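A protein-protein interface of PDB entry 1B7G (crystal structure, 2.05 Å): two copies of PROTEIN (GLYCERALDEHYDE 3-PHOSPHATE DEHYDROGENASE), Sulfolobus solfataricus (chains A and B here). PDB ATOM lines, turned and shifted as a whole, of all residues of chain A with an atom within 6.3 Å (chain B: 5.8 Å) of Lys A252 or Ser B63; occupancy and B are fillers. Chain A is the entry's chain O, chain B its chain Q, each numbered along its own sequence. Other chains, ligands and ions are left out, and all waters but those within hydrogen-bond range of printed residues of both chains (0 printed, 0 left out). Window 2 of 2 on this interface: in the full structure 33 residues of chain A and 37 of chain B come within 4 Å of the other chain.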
ATOM      1  N   SER A 250      19.161   2.021 -28.066  1.00  0.00           N
ATOM      2  CA  SER A 250      19.827   1.617 -26.842  1.00  0.00           C
ATOM      3  C   SER A 250      21.337   1.824 -26.963  1.00  0.00           C
ATOM      4  O   SER A 250      21.843   2.149 -28.028  1.00  0.00           O
ATOM      5  CB  SER A 250      19.529   0.137 -26.542  1.00  0.00           C
ATOM      6  OG  SER A 250      20.341  -0.739 -27.316  1.00  0.00           O
ATOM      7  N   SER A 251      22.065   1.538 -25.886  1.00  0.00           N
ATOM      8  CA  SER A 251      23.542   1.610 -25.969  1.00  0.00           C
ATOM      9  C   SER A 251      24.098   0.198 -25.864  1.00  0.00           C
ATOM     10  O   SER A 251      25.230  -0.017 -25.464  1.00  0.00           O
ATOM     11  CB  SER A 251      24.020   2.458 -24.766  1.00  0.00           C
ATOM     12  OG  SER A 251      23.512   1.848 -23.589  1.00  0.00           O
ATOM     13  N   LYS A 252      23.282  -0.802 -26.175  1.00  0.00           N
ATOM     14  CA  LYS A 252      23.679  -2.199 -26.038  1.00  0.00           C
ATOM     15  C   LYS A 252      24.554  -2.724 -27.162  1.00  0.00           C
ATOM     16  O   LYS A 252      25.387  -3.611 -26.968  1.00  0.00           O
ATOM     17  CB  LYS A 252      22.391  -3.029 -25.937  1.00  0.00           C
ATOM     18  CG  LYS A 252      22.575  -4.508 -25.666  1.00  0.00           C
ATOM     19  CD  LYS A 252      21.245  -5.112 -25.205  1.00  0.00           C
ATOM     20  CE  LYS A 252      21.419  -6.555 -24.777  1.00  0.00           C
ATOM     21  NZ  LYS A 252      20.101  -7.233 -24.559  1.00  0.00           N
ATOM     22  N   TYR A 253      24.285  -2.250 -28.375  1.00  0.00           N
ATOM     23  CA  TYR A 253      24.996  -2.812 -29.534  1.00  0.00           C
ATOM     24  C   TYR A 253      25.946  -1.858 -30.188  1.00  0.00           C
ATOM     25  O   TYR A 253      26.244  -2.017 -31.384  1.00  0.00           O
ATOM     26  CB  TYR A 253      23.928  -3.367 -30.481  1.00  0.00           C
ATOM     27  CG  TYR A 253      23.046  -4.406 -29.801  1.00  0.00           C
ATOM     28  CD1 TYR A 253      23.583  -5.643 -29.473  1.00  0.00           C
ATOM     29  CD2 TYR A 253      21.704  -4.156 -29.549  1.00  0.00           C
ATOM     30  CE1 TYR A 253      22.809  -6.623 -28.888  1.00  0.00           C
ATOM     31  CE2 TYR A 253      20.898  -5.130 -28.963  1.00  0.00           C
ATOM     32  CZ  TYR A 253      21.464  -6.350 -28.651  1.00  0.00           C
ATOM     33  OH  TYR A 253      20.699  -7.310 -28.068  1.00  0.00           O
ATOM     34  N   ASP A 254      26.485  -0.885 -29.439  1.00  0.00           N
ATOM     35  CA  ASP A 254      27.501  -0.020 -30.081  1.00  0.00           C
ATOM     36  C   ASP A 254      26.971   0.639 -31.329  1.00  0.00           C
ATOM     37  O   ASP A 254      27.693   0.712 -32.330  1.00  0.00           O
ATOM     38  CB  ASP A 254      28.804  -0.806 -30.299  1.00  0.00           C
ATOM     39  CG  ASP A 254      30.016   0.124 -30.355  1.00  0.00           C
ATOM     40  OD1 ASP A 254      29.915   1.332 -30.049  1.00  0.00           O
ATOM     41  OD2 ASP A 254      31.091  -0.366 -30.779  1.00  0.00           O
ATOM     42  N   ALA A 255      25.758   1.219 -31.325  1.00  0.00           N
ATOM     43  CA  ALA A 255      25.284   1.863 -32.541  1.00  0.00           C
ATOM     44  C   ALA A 255      24.867   3.323 -32.331  1.00  0.00           C
ATOM     45  O   ALA A 255      24.065   3.857 -33.109  1.00  0.00           O
ATOM     46  CB  ALA A 255      24.130   1.070 -33.196  1.00  0.00           C
ATOM     47  N   GLU A 256      25.348   4.002 -31.293  1.00  0.00           N
ATOM     48  CA  GLU A 256      24.943   5.370 -31.004  1.00  0.00           C
ATOM     49  C   GLU A 256      25.767   6.454 -31.690  1.00  0.00           C
ATOM     50  O   GLU A 256      26.508   7.214 -31.065  1.00  0.00           O
ATOM     51  CB  GLU A 256      24.986   5.648 -29.505  1.00  0.00           C
ATOM     52  CG  GLU A 256      24.206   4.670 -28.645  1.00  0.00           C
ATOM     53  CD  GLU A 256      24.516   5.007 -27.181  1.00  0.00           C
ATOM     54  OE1 GLU A 256      25.572   4.545 -26.732  1.00  0.00           O
ATOM     55  OE2 GLU A 256      23.733   5.741 -26.576  1.00  0.00           O
ATOM     56  N   ILE A 340      17.396  -0.530 -32.278  1.00  0.00           N
ATOM     57  CA  ILE A 340      18.690  -1.145 -31.984  1.00  0.00           C
ATOM     58  C   ILE A 340      19.124  -0.712 -30.600  1.00  0.00           C
ATOM     59  O   ILE A 340      18.418   0.120 -29.954  1.00  0.00           O
ATOM     60  CB  ILE A 340      19.736  -0.779 -33.057  1.00  0.00           C
ATOM     61  CG1 ILE A 340      20.976  -1.662 -32.974  1.00  0.00           C
ATOM     62  CG2 ILE A 340      20.149   0.695 -32.945  1.00  0.00           C
ATOM     63  CD1 ILE A 340      20.715  -3.137 -33.231  1.00  0.00           C
ATOM     64  OXT ILE A 340      20.111  -1.254 -30.058  1.00  0.00           O
ATOM     65  N   PRO B  36      29.529  -8.634 -29.794  1.00  0.00           N
ATOM     66  CA  PRO B  36      28.088  -8.620 -30.066  1.00  0.00           C
ATOM     67  C   PRO B  36      27.624  -7.248 -30.463  1.00  0.00           C
ATOM     68  O   PRO B  36      26.797  -6.681 -29.727  1.00  0.00           O
ATOM     69  CB  PRO B  36      27.554  -9.188 -28.781  1.00  0.00           C
ATOM     70  CG  PRO B  36      28.469  -8.627 -27.722  1.00  0.00           C
ATOM     71  CD  PRO B  36      29.830  -8.700 -28.344  1.00  0.00           C
ATOM     72  N   ASN B  37      28.080  -6.621 -31.539  1.00  0.00           N
ATOM     73  CA  ASN B  37      27.600  -5.270 -31.877  1.00  0.00           C
ATOM     74  C   ASN B  37      26.285  -5.376 -32.618  1.00  0.00           C
ATOM     75  O   ASN B  37      25.708  -6.480 -32.782  1.00  0.00           O
ATOM     76  CB  ASN B  37      28.682  -4.555 -32.710  1.00  0.00           C
ATOM     77  CG  ASN B  37      28.797  -5.021 -34.129  1.00  0.00           C
ATOM     78  OD1 ASN B  37      28.472  -6.188 -34.398  1.00  0.00           O
ATOM     79  ND2 ASN B  37      29.225  -4.170 -35.063  1.00  0.00           N
ATOM     80  N   LYS B  59      31.377 -13.167 -22.331  1.00  0.00           N
ATOM     81  CA  LYS B  59      31.143 -11.756 -22.598  1.00  0.00           C
ATOM     82  C   LYS B  59      30.056 -11.568 -23.644  1.00  0.00           C
ATOM     83  O   LYS B  59      29.075 -10.869 -23.417  1.00  0.00           O
ATOM     84  CB  LYS B  59      32.429 -11.044 -23.019  1.00  0.00           C
ATOM     85  CG  LYS B  59      32.364  -9.529 -22.921  1.00  0.00           C
ATOM     86  CD  LYS B  59      33.699  -8.865 -23.211  1.00  0.00           C
ATOM     87  CE  LYS B  59      34.745  -9.138 -22.146  1.00  0.00           C
ATOM     88  NZ  LYS B  59      35.939  -8.253 -22.277  1.00  0.00           N
ATOM     89  N   PHE B  60      30.226 -12.230 -24.786  1.00  0.00           N
ATOM     90  CA  PHE B  60      29.273 -12.132 -25.881  1.00  0.00           C
ATOM     91  C   PHE B  60      27.866 -12.518 -25.463  1.00  0.00           C
ATOM     92  O   PHE B  60      26.918 -11.888 -25.909  1.00  0.00           O
ATOM     93  CB  PHE B  60      29.711 -13.068 -27.011  1.00  0.00           C
ATOM     94  CG  PHE B  60      29.050 -12.834 -28.331  1.00  0.00           C
ATOM     95  CD1 PHE B  60      27.746 -13.225 -28.586  1.00  0.00           C
ATOM     96  CD2 PHE B  60      29.774 -12.217 -29.341  1.00  0.00           C
ATOM     97  CE1 PHE B  60      27.193 -13.001 -29.840  1.00  0.00           C
ATOM     98  CE2 PHE B  60      29.214 -11.992 -30.579  1.00  0.00           C
ATOM     99  CZ  PHE B  60      27.917 -12.380 -30.814  1.00  0.00           C
ATOM    100  N   GLU B  61      27.731 -13.569 -24.673  1.00  0.00           N
ATOM    101  CA  GLU B  61      26.496 -14.143 -24.212  1.00  0.00           C
ATOM    102  C   GLU B  61      25.682 -13.277 -23.266  1.00  0.00           C
ATOM    103  O   GLU B  61      24.485 -13.517 -23.066  1.00  0.00           O
ATOM    104  CB  GLU B  61      26.750 -15.505 -23.536  1.00  0.00           C
ATOM    105  CG  GLU B  61      26.732 -16.676 -24.511  1.00  0.00           C
ATOM    106  CD  GLU B  61      26.764 -18.014 -23.792  1.00  0.00           C
ATOM    107  OE1 GLU B  61      26.888 -18.010 -22.546  1.00  0.00           O
ATOM    108  OE2 GLU B  61      26.665 -19.064 -24.454  1.00  0.00           O
ATOM    109  N   GLU B  62      26.285 -12.252 -22.696  1.00  0.00           N
ATOM    110  CA  GLU B  62      25.639 -11.291 -21.831  1.00  0.00           C
ATOM    111  C   GLU B  62      24.655 -10.431 -22.609  1.00  0.00           C
ATOM    112  O   GLU B  62      23.688  -9.930 -22.037  1.00  0.00           O
ATOM    113  CB  GLU B  62      26.701 -10.373 -21.203  1.00  0.00           C
ATOM    114  CG  GLU B  62      27.602 -11.080 -20.201  1.00  0.00           C
ATOM    115  CD  GLU B  62      28.791 -10.235 -19.793  1.00  0.00           C
ATOM    116  OE1 GLU B  62      28.787  -9.015 -20.056  1.00  0.00           O
ATOM    117  OE2 GLU B  62      29.752 -10.791 -19.219  1.00  0.00           O
ATOM    118  N   SER B  63      24.880 -10.234 -23.906  1.00  0.00           N
ATOM    119  CA  SER B  63      24.003  -9.388 -24.696  1.00  0.00           C
ATOM    120  C   SER B  63      22.707 -10.068 -25.094  1.00  0.00           C
ATOM    121  O   SER B  63      21.901  -9.420 -25.781  1.00  0.00           O
ATOM    122  CB  SER B  63      24.719  -8.948 -25.984  1.00  0.00           C
ATOM    123  OG  SER B  63      24.867 -10.072 -26.843  1.00  0.00           O
ATOM    124  N   GLY B  64      22.549 -11.358 -24.855  1.00  0.00           N
ATOM    125  CA  GLY B  64      21.350 -12.074 -25.264  1.00  0.00           C
ATOM    126  C   GLY B  64      21.440 -12.746 -26.624  1.00  0.00           C
ATOM    127  O   GLY B  64      20.548 -13.568 -26.934  1.00  0.00           O
ATOM    128  N   ILE B  65      22.387 -12.380 -27.474  1.00  0.00           N
ATOM    129  CA  ILE B  65      22.530 -13.040 -28.775  1.00  0.00           C
ATOM    130  C   ILE B  65      23.079 -14.448 -28.531  1.00  0.00           C
ATOM    131  O   ILE B  65      24.140 -14.527 -27.920  1.00  0.00           O
ATOM    132  CB  ILE B  65      23.538 -12.299 -29.673  1.00  0.00           C
ATOM    133  CG1 ILE B  65      23.116 -10.826 -29.779  1.00  0.00           C
ATOM    134  CG2 ILE B  65      23.673 -12.947 -31.041  1.00  0.00           C
ATOM    135  CD1 ILE B  65      23.939  -9.993 -30.698  1.00  0.00           C
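Of the 8 printed residues of chain A, 2 touch a printed residue of chain B.
Printed residues of chain A that touch a printed residue of chain B: Lys A252 and Tyr A253.
Hydrophobic or aromatic side chains of chain A within 4 Å of the printed part of chain B: Tyr A253.
Printed residues of chain B that touch a printed residue of chain A: Pro B36, Asn B37, Ser B63 and Ile B65.
Hydrophobic or aromatic side chains of chain B within 4 Å of the printed part of chain A: Ile B65.
Among the printed residues, no Asp or Glu carboxylate lies within 4 Å of a Lys or Arg side-chain nitrogen of the other chain.
Of chain B, only Ser B63 (3.1 Å) comes within 4 Å of Lys A252.
Of the printed residues of chain B, Tyr A253 touches Pro B36, Asn B37, Ser B63 and Ile B65.
Asp A254 touches none of the printed residues of chain B.
Printed residues of chain A within 4 Å of Pro B36: Tyr A253.
Of the printed residues of chain A, Asn B37 touches Tyr A253 (3.6 Å).
Ser B63 touches just these residues of chain A: Lys A252 and Tyr A253.
Of the printed residues of chain A, Ile B65 touches Tyr A253.
The nearest residue of chain B that does not touch Lys A252 is Pro B36 (4.4 Å).
The nearest printed residue of chain B that does not touch Tyr A253 is Gly B64 (5.5 Å).
No position is printed for both chains.
Of the 5 pairs that touch across the chains among the printed residues, none has its exchanged pair printed and touching as well.
The side-chain hydroxyl (OG) of Ser A250 is in hydrogen-bond range of the backbone NH (N) of Lys A252 (3.2 Å).
The side-chain hydroxyl (OG) of Ser B63 sits at hydrogen-bond distance from the backbone carbonyl oxygen (O) of Phe B60 (2.9 Å).
N of Ile B65 lies close to OG of Ser B63 (3.4 Å).
Among the printed residues, pairs that only touch across the chains: Tyr A253 with Pro B36, Tyr A253 with Asn B37 and Tyr A253 with Ile B65.
The side-chain hydroxyl of Tyr A253 is in hydrogen-bond range of the backbone carbonyl oxygen of Ser B63, 3.3 Å away.
The backbone carbonyl oxygen of Ser B63 lies close to the side-chain amino group of Lys A252 (3.1 Å).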
